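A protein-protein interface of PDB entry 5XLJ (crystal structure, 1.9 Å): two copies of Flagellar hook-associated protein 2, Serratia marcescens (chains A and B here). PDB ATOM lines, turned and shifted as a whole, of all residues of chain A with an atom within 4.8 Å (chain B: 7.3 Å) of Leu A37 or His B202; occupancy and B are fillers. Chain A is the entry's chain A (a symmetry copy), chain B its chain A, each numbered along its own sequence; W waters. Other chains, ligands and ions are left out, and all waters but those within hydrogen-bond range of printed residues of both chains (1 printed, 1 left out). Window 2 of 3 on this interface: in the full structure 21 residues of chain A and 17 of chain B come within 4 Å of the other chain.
The backbone carbonyl oxygen of Leu A37 sits at hydrogen-bond distance from the side-chain amide nitrogen of Gln A162, 2.7 Å away.
The backbone NH (N) of Ala A38 sits at hydrogen-bond distance from the side-chain amide oxygen (OD1) of Asn A178, 2.8 Å away.
N of Gln A39 is in hydrogen-bond range of O of Gln A162, 2.9 Å away.
Among the printed residues, merely in contact across the chains: Leu A37 with His B202 (3.6 Å), Ala A38 with His B202 (3.2 Å), Gln A39 with His B202 (3.9 Å) and Lys A194 with Glu B199 (3.8 Å).
Leu A37 touches just one residue of chain B: His B202 (3.6 Å).
Of the printed residues of chain B, Gln A39 touches His B202.
Of the printed residues of chain B, Lys A194 touches Glu B199 (3.8 Å).
Phe B17 touches none of the printed residues of chain A.
Val B32 touches none of the printed residues of chain A.
Printed residues of chain A within 4 Å of Glu B199: Lys A194.
Of chain A, only Leu A37 (3.6 Å), Ala A38 (3.2 Å) and Gln A39 (3.9 Å) come within 4 Å of His B202.
The nearest residue of chain A that does not touch His B202 is Asn A178 (4.2 Å).
Of the 14 printed residues of chain A, 4 touch a printed residue of chain B.
Along chain A the printed residues that touch a printed residue of chain B span positions 37 to 194.
Of the 11 printed residues of chain B, 2 touch a printed residue of chain A.
Hydrophobic or aromatic side chains of chain B that line the printed part of chain A: His B202.
Among the printed residues, 4 pairs touch across the chains.
No position is printed for both chains.
Of the 4 pairs that touch across the chains among the printed residues, none has its exchanged pair printed and touching as well.
Water W1 bridges NE2 of His B202 and OE1 of Gln A39.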
ATOM      1  N   VAL A  34     -20.135 -34.581 -24.251  1.00  0.00           N
ATOM      2  CA  VAL A  34     -19.498 -33.263 -24.256  1.00  0.00           C
ATOM      3  C   VAL A  34     -17.996 -33.488 -24.211  1.00  0.00           C
ATOM      4  O   VAL A  34     -17.462 -33.998 -23.214  1.00  0.00           O
ATOM      5  CB  VAL A  34     -19.961 -32.395 -23.092  1.00  0.00           C
ATOM      6  CG1 VAL A  34     -19.360 -30.966 -23.188  1.00  0.00           C
ATOM      7  CG2 VAL A  34     -21.493 -32.343 -23.068  1.00  0.00           C
ATOM      8  N   ASN A  35     -17.325 -33.151 -25.309  1.00  0.00           N
ATOM      9  CA  ASN A  35     -15.902 -33.456 -25.480  1.00  0.00           C
ATOM     10  C   ASN A  35     -14.985 -32.275 -25.162  1.00  0.00           C
ATOM     11  O   ASN A  35     -13.851 -32.474 -24.719  1.00  0.00           O
ATOM     12  CB  ASN A  35     -15.682 -34.032 -26.883  1.00  0.00           C
ATOM     13  CG  ASN A  35     -16.422 -35.387 -27.067  1.00  0.00           C
ATOM     14  OD1 ASN A  35     -16.409 -36.233 -26.167  1.00  0.00           O
ATOM     15  ND2 ASN A  35     -17.123 -35.547 -28.182  1.00  0.00           N
ATOM     16  N   LYS A  36     -15.495 -31.058 -25.339  1.00  0.00           N
ATOM     17  CA  LYS A  36     -14.728 -29.827 -25.074  1.00  0.00           C
ATOM     18  C   LYS A  36     -15.690 -28.678 -24.720  1.00  0.00           C
ATOM     19  O   LYS A  36     -16.776 -28.604 -25.275  1.00  0.00           O
ATOM     20  CB  LYS A  36     -13.902 -29.409 -26.305  1.00  0.00           C
ATOM     21  CG  LYS A  36     -12.535 -30.103 -26.424  1.00  0.00           C
ATOM     22  N   LEU A  37     -15.275 -27.803 -23.806  1.00  0.00           N
ATOM     23  CA  LEU A  37     -16.023 -26.600 -23.499  1.00  0.00           C
ATOM     24  C   LEU A  37     -15.345 -25.434 -24.220  1.00  0.00           C
ATOM     25  O   LEU A  37     -14.127 -25.417 -24.361  1.00  0.00           O
ATOM     26  CB  LEU A  37     -16.020 -26.336 -21.998  1.00  0.00           C
ATOM     27  CG  LEU A  37     -16.694 -27.360 -21.099  1.00  0.00           C
ATOM     28  CD1 LEU A  37     -16.517 -26.991 -19.594  1.00  0.00           C
ATOM     29  CD2 LEU A  37     -18.114 -27.442 -21.445  1.00  0.00           C
ATOM     30  N   ALA A  38     -16.147 -24.488 -24.699  1.00  0.00           N
ATOM     31  CA  ALA A  38     -15.636 -23.238 -25.237  1.00  0.00           C
ATOM     32  C   ALA A  38     -14.820 -22.493 -24.175  1.00  0.00           C
ATOM     33  O   ALA A  38     -15.198 -22.483 -22.993  1.00  0.00           O
ATOM     34  CB  ALA A  38     -16.781 -22.381 -25.695  1.00  0.00           C
ATOM     35  N   GLN A  39     -13.705 -21.900 -24.606  1.00  0.00           N
ATOM     36  CA  GLN A  39     -12.816 -21.140 -23.723  1.00  0.00           C
ATOM     37  C   GLN A  39     -12.509 -19.819 -24.355  1.00  0.00           C
ATOM     38  O   GLN A  39     -12.392 -19.713 -25.593  1.00  0.00           O
ATOM     39  CB  GLN A  39     -11.451 -21.822 -23.472  1.00  0.00           C
ATOM     40  CG  GLN A  39     -11.505 -23.125 -22.803  1.00  0.00           C
ATOM     41  CD  GLN A  39     -10.133 -23.718 -22.464  1.00  0.00           C
ATOM     42  OE1 GLN A  39     -10.050 -24.552 -21.578  1.00  0.00           O
ATOM     43  NE2 GLN A  39      -9.090 -23.337 -23.179  1.00  0.00           N
ATOM     44  N   GLN A 162     -10.895 -21.800 -27.623  1.00  0.00           N
ATOM     45  CA  GLN A 162     -11.419 -23.125 -27.916  1.00  0.00           C
ATOM     46  C   GLN A 162     -12.902 -23.060 -28.164  1.00  0.00           C
ATOM     47  O   GLN A 162     -13.603 -22.269 -27.514  1.00  0.00           O
ATOM     48  CB  GLN A 162     -11.167 -24.015 -26.687  1.00  0.00           C
ATOM     49  CG  GLN A 162     -11.448 -25.445 -26.803  1.00  0.00           C
ATOM     50  CD  GLN A 162     -10.831 -26.199 -25.619  1.00  0.00           C
ATOM     51  OE1 GLN A 162      -9.647 -26.519 -25.641  1.00  0.00           O
ATOM     52  NE2 GLN A 162     -11.623 -26.447 -24.585  1.00  0.00           N
ATOM     53  N   ASP A 163     -13.378 -23.894 -29.086  1.00  0.00           N
ATOM     54  CA  ASP A 163     -14.804 -24.110 -29.285  1.00  0.00           C
ATOM     55  C   ASP A 163     -15.348 -25.201 -28.360  1.00  0.00           C
ATOM     56  O   ASP A 163     -14.624 -26.090 -27.903  1.00  0.00           O
ATOM     57  CB  ASP A 163     -15.096 -24.525 -30.732  1.00  0.00           C
ATOM     58  CG  ASP A 163     -15.347 -23.344 -31.680  1.00  0.00           C
ATOM     59  OD1 ASP A 163     -15.188 -22.176 -31.306  1.00  0.00           O
ATOM     60  OD2 ASP A 163     -15.727 -23.607 -32.838  1.00  0.00           O
ATOM     61  N   ALA A 164     -16.647 -25.127 -28.113  1.00  0.00           N
ATOM     62  CA  ALA A 164     -17.380 -26.218 -27.505  1.00  0.00           C
ATOM     63  C   ALA A 164     -17.496 -27.314 -28.566  1.00  0.00           C
ATOM     64  O   ALA A 164     -17.675 -27.023 -29.758  1.00  0.00           O
ATOM     65  CB  ALA A 164     -18.776 -25.742 -27.031  1.00  0.00           C
ATOM     66  N   ASN A 178     -20.740 -21.906 -24.908  1.00  0.00           N
ATOM     67  CA  ASN A 178     -21.253 -23.009 -24.145  1.00  0.00           C
ATOM     68  C   ASN A 178     -22.772 -22.988 -23.999  1.00  0.00           C
ATOM     69  O   ASN A 178     -23.329 -23.783 -23.243  1.00  0.00           O
ATOM     70  CB  ASN A 178     -20.545 -23.048 -22.771  1.00  0.00           C
ATOM     71  CG  ASN A 178     -19.089 -23.390 -22.927  1.00  0.00           C
ATOM     72  OD1 ASN A 178     -18.771 -24.345 -23.660  1.00  0.00           O
ATOM     73  ND2 ASN A 178     -18.187 -22.603 -22.301  1.00  0.00           N
ATOM     74  N   LEU A 191     -23.756 -25.948 -21.595  1.00  0.00           N
ATOM     75  CA  LEU A 191     -22.714 -26.875 -21.165  1.00  0.00           C
ATOM     76  C   LEU A 191     -22.080 -26.466 -19.869  1.00  0.00           C
ATOM     77  O   LEU A 191     -21.731 -25.287 -19.684  1.00  0.00           O
ATOM     78  CB  LEU A 191     -21.613 -26.980 -22.223  1.00  0.00           C
ATOM     79  CG  LEU A 191     -22.066 -27.404 -23.603  1.00  0.00           C
ATOM     80  CD1 LEU A 191     -20.898 -27.407 -24.553  1.00  0.00           C
ATOM     81  CD2 LEU A 191     -22.765 -28.785 -23.549  1.00  0.00           C
ATOM     82  N   LYS A 192     -21.888 -27.442 -18.979  1.00  0.00           N
ATOM     83  CA  LYS A 192     -21.254 -27.190 -17.683  1.00  0.00           C
ATOM     84  C   LYS A 192     -19.898 -27.883 -17.551  1.00  0.00           C
ATOM     85  O   LYS A 192     -18.949 -27.283 -17.064  1.00  0.00           O
ATOM     86  CB  LYS A 192     -22.191 -27.619 -16.559  1.00  0.00           C
ATOM     87  CG  LYS A 192     -23.607 -27.016 -16.640  1.00  0.00           C
ATOM     88  CD  LYS A 192     -23.625 -25.488 -16.415  1.00  0.00           C
ATOM     89  CE  LYS A 192     -24.994 -24.857 -16.763  1.00  0.00           C
ATOM     90  NZ  LYS A 192     -24.911 -23.362 -16.669  1.00  0.00           N
ATOM     91  N   THR A 193     -19.811 -29.139 -17.986  1.00  0.00           N
ATOM     92  CA  THR A 193     -18.575 -29.910 -17.924  1.00  0.00           C
ATOM     93  C   THR A 193     -18.545 -30.911 -19.072  1.00  0.00           C
ATOM     94  O   THR A 193     -19.541 -31.106 -19.784  1.00  0.00           O
ATOM     95  CB  THR A 193     -18.417 -30.697 -16.563  1.00  0.00           C
ATOM     96  OG1 THR A 193     -19.316 -31.808 -16.522  1.00  0.00           O
ATOM     97  CG2 THR A 193     -18.680 -29.814 -15.348  1.00  0.00           C
ATOM     98  N   LYS A 194     -17.401 -31.559 -19.246  1.00  0.00           N
ATOM     99  CA  LYS A 194     -17.318 -32.684 -20.155  1.00  0.00           C
ATOM    100  C   LYS A 194     -18.110 -33.855 -19.577  1.00  0.00           C
ATOM    101  O   LYS A 194     -18.322 -33.942 -18.366  1.00  0.00           O
ATOM    102  CB  LYS A 194     -15.872 -33.145 -20.301  1.00  0.00           C
ATOM    103  CG  LYS A 194     -14.920 -32.170 -20.921  1.00  0.00           C
ATOM    104  CD  LYS A 194     -13.579 -32.884 -21.152  1.00  0.00           C
ATOM    105  CE  LYS A 194     -12.459 -31.939 -21.340  1.00  0.00           C
ATOM    106  NZ  LYS A 194     -11.182 -32.692 -21.273  1.00  0.00           N
ATOM    107  N   PHE B  17     -14.537 -25.887  -6.009  1.00  0.00           N
ATOM    108  CA  PHE B  17     -14.301 -24.689  -5.190  1.00  0.00           C
ATOM    109  C   PHE B  17     -15.518 -23.788  -5.090  1.00  0.00           C
ATOM    110  O   PHE B  17     -16.397 -23.808  -5.957  1.00  0.00           O
ATOM    111  CB  PHE B  17     -13.107 -23.879  -5.716  1.00  0.00           C
ATOM    112  CG  PHE B  17     -13.233 -23.470  -7.158  1.00  0.00           C
ATOM    113  CD1 PHE B  17     -13.922 -22.320  -7.508  1.00  0.00           C
ATOM    114  CD2 PHE B  17     -12.673 -24.245  -8.165  1.00  0.00           C
ATOM    115  CE1 PHE B  17     -14.058 -21.949  -8.843  1.00  0.00           C
ATOM    116  CE2 PHE B  17     -12.813 -23.880  -9.505  1.00  0.00           C
ATOM    117  CZ  PHE B  17     -13.495 -22.728  -9.832  1.00  0.00           C
ATOM    118  N   ASN B  29     -14.359 -14.001 -18.061  1.00  0.00           N
ATOM    119  CA  ASN B  29     -14.287 -15.446 -18.235  1.00  0.00           C
ATOM    120  C   ASN B  29     -13.042 -15.983 -17.546  1.00  0.00           C
ATOM    121  O   ASN B  29     -11.953 -15.498 -17.809  1.00  0.00           O
ATOM    122  CB  ASN B  29     -14.261 -15.763 -19.728  1.00  0.00           C
ATOM    123  CG  ASN B  29     -15.551 -15.340 -20.432  1.00  0.00           C
ATOM    124  OD1 ASN B  29     -16.650 -15.680 -19.986  1.00  0.00           O
ATOM    125  ND2 ASN B  29     -15.419 -14.573 -21.495  1.00  0.00           N
ATOM    126  N   TYR B  30     -13.213 -16.982 -16.681  1.00  0.00           N
ATOM    127  CA  TYR B  30     -12.109 -17.640 -15.978  1.00  0.00           C
ATOM    128  C   TYR B  30     -12.170 -19.160 -16.106  1.00  0.00           C
ATOM    129  O   TYR B  30     -13.256 -19.724 -16.179  1.00  0.00           O
ATOM    130  CB  TYR B  30     -12.095 -17.242 -14.491  1.00  0.00           C
ATOM    131  CG  TYR B  30     -12.007 -15.748 -14.309  1.00  0.00           C
ATOM    132  CD1 TYR B  30     -13.148 -14.964 -14.384  1.00  0.00           C
ATOM    133  CD2 TYR B  30     -10.781 -15.115 -14.091  1.00  0.00           C
ATOM    134  CE1 TYR B  30     -13.094 -13.583 -14.260  1.00  0.00           C
ATOM    135  CE2 TYR B  30     -10.714 -13.721 -13.939  1.00  0.00           C
ATOM    136  CZ  TYR B  30     -11.884 -12.961 -14.035  1.00  0.00           C
ATOM    137  OH  TYR B  30     -11.859 -11.573 -13.921  1.00  0.00           O
ATOM    138  N   VAL B  31     -10.999 -19.801 -16.165  1.00  0.00           N
ATOM    139  CA  VAL B  31     -10.904 -21.245 -16.023  1.00  0.00           C
ATOM    140  C   VAL B  31      -9.953 -21.525 -14.866  1.00  0.00           C
ATOM    141  O   VAL B  31      -8.937 -20.827 -14.694  1.00  0.00           O
ATOM    142  CB  VAL B  31     -10.487 -21.974 -17.347  1.00  0.00           C
ATOM    143  CG1 VAL B  31     -11.559 -21.752 -18.453  1.00  0.00           C
ATOM    144  CG2 VAL B  31      -9.147 -21.483 -17.852  1.00  0.00           C
ATOM    145  N   VAL B  32     -10.296 -22.506 -14.046  1.00  0.00           N
ATOM    146  CA  VAL B  32      -9.505 -22.826 -12.857  1.00  0.00           C
ATOM    147  C   VAL B  32      -9.175 -24.318 -12.823  1.00  0.00           C
ATOM    148  O   VAL B  32     -10.055 -25.162 -13.086  1.00  0.00           O
ATOM    149  CB  VAL B  32     -10.236 -22.418 -11.570  1.00  0.00           C
ATOM    150  CG1 VAL B  32      -9.408 -22.779 -10.325  1.00  0.00           C
ATOM    151  CG2 VAL B  32     -10.540 -20.907 -11.558  1.00  0.00           C
ATOM    152  N   GLU B 199      -9.378 -31.254 -17.195  1.00  0.00           N
ATOM    153  CA  GLU B 199     -10.756 -30.802 -17.031  1.00  0.00           C
ATOM    154  C   GLU B 199     -10.836 -29.532 -16.166  1.00  0.00           C
ATOM    155  O   GLU B 199     -11.351 -29.552 -15.047  1.00  0.00           O
ATOM    156  CB  GLU B 199     -11.576 -31.951 -16.426  1.00  0.00           C
ATOM    157  CG  GLU B 199     -13.024 -32.000 -16.862  1.00  0.00           C
ATOM    158  CD  GLU B 199     -13.609 -33.413 -16.916  1.00  0.00           C
ATOM    159  OE1 GLU B 199     -14.827 -33.563 -16.672  1.00  0.00           O
ATOM    160  OE2 GLU B 199     -12.873 -34.376 -17.223  1.00  0.00           O
ATOM    161  N   PRO B 200     -10.333 -28.412 -16.693  1.00  0.00           N
ATOM    162  CA  PRO B 200     -10.444 -27.161 -15.940  1.00  0.00           C
ATOM    163  C   PRO B 200     -11.910 -26.781 -15.690  1.00  0.00           C
ATOM    164  O   PRO B 200     -12.772 -27.095 -16.524  1.00  0.00           O
ATOM    165  CB  PRO B 200      -9.778 -26.147 -16.864  1.00  0.00           C
ATOM    166  CG  PRO B 200      -9.865 -26.722 -18.193  1.00  0.00           C
ATOM    167  CD  PRO B 200      -9.785 -28.188 -18.043  1.00  0.00           C
ATOM    168  N   GLN B 201     -12.188 -26.148 -14.548  1.00  0.00           N
ATOM    169  CA  GLN B 201     -13.548 -25.717 -14.225  1.00  0.00           C
ATOM    170  C   GLN B 201     -13.787 -24.248 -14.594  1.00  0.00           C
ATOM    171  O   GLN B 201     -12.930 -23.378 -14.381  1.00  0.00           O
ATOM    172  CB  GLN B 201     -13.892 -26.035 -12.766  1.00  0.00           C
ATOM    173  CG  GLN B 201     -14.100 -27.572 -12.556  1.00  0.00           C
ATOM    174  CD  GLN B 201     -14.535 -27.992 -11.139  1.00  0.00           C
ATOM    175  OE1 GLN B 201     -14.834 -27.153 -10.296  1.00  0.00           O
ATOM    176  NE2 GLN B 201     -14.585 -29.317 -10.890  1.00  0.00           N
ATOM    177  N   HIS B 202     -14.945 -23.982 -15.177  1.00  0.00           N
ATOM    178  CA  HIS B 202     -15.246 -22.663 -15.712  1.00  0.00           C
ATOM    179  C   HIS B 202     -15.947 -21.782 -14.679  1.00  0.00           C
ATOM    180  O   HIS B 202     -16.719 -22.257 -13.830  1.00  0.00           O
ATOM    181  CB  HIS B 202     -16.042 -22.795 -16.998  1.00  0.00           C
ATOM    182  CG  HIS B 202     -15.238 -23.376 -18.115  1.00  0.00           C
ATOM    183  ND1 HIS B 202     -15.190 -22.821 -19.372  1.00  0.00           N
ATOM    184  CD2 HIS B 202     -14.406 -24.444 -18.142  1.00  0.00           C
ATOM    185  CE1 HIS B 202     -14.376 -23.534 -20.130  1.00  0.00           C
ATOM    186  NE2 HIS B 202     -13.888 -24.525 -19.407  1.00  0.00           N
ATOM    187  N   LEU B 203     -15.624 -20.497 -14.734  1.00  0.00           N
ATOM    188  CA  LEU B 203     -16.155 -19.518 -13.809  1.00  0.00           C
ATOM    189  C   LEU B 203     -16.442 -18.248 -14.607  1.00  0.00           C
ATOM    190  O   LEU B 203     -15.577 -17.772 -15.335  1.00  0.00           O
ATOM    191  CB  LEU B 203     -15.144 -19.245 -12.695  1.00  0.00           C
ATOM    192  CG  LEU B 203     -15.423 -18.058 -11.759  1.00  0.00           C
ATOM    193  CD1 LEU B 203     -16.643 -18.317 -10.896  1.00  0.00           C
ATOM    194  CD2 LEU B 203     -14.212 -17.762 -10.895  1.00  0.00           C
ATOM    195  N   VAL B 204     -17.664 -17.731 -14.505  1.00  0.00           N
ATOM    196  CA  VAL B 204     -17.972 -16.410 -15.057  1.00  0.00           C
ATOM    197  C   VAL B 204     -18.283 -15.476 -13.892  1.00  0.00           C
ATOM    198  O   VAL B 204     -19.142 -15.781 -13.060  1.00  0.00           O
ATOM    199  CB  VAL B 204     -19.159 -16.444 -16.044  1.00  0.00           C
ATOM    200  CG1 VAL B 204     -19.422 -15.034 -16.627  1.00  0.00           C
ATOM    201  CG2 VAL B 204     -18.890 -17.444 -17.168  1.00  0.00           C
HETATM  202  O   HOH W   1     -12.132 -25.944 -20.539  1.00  0.00           O
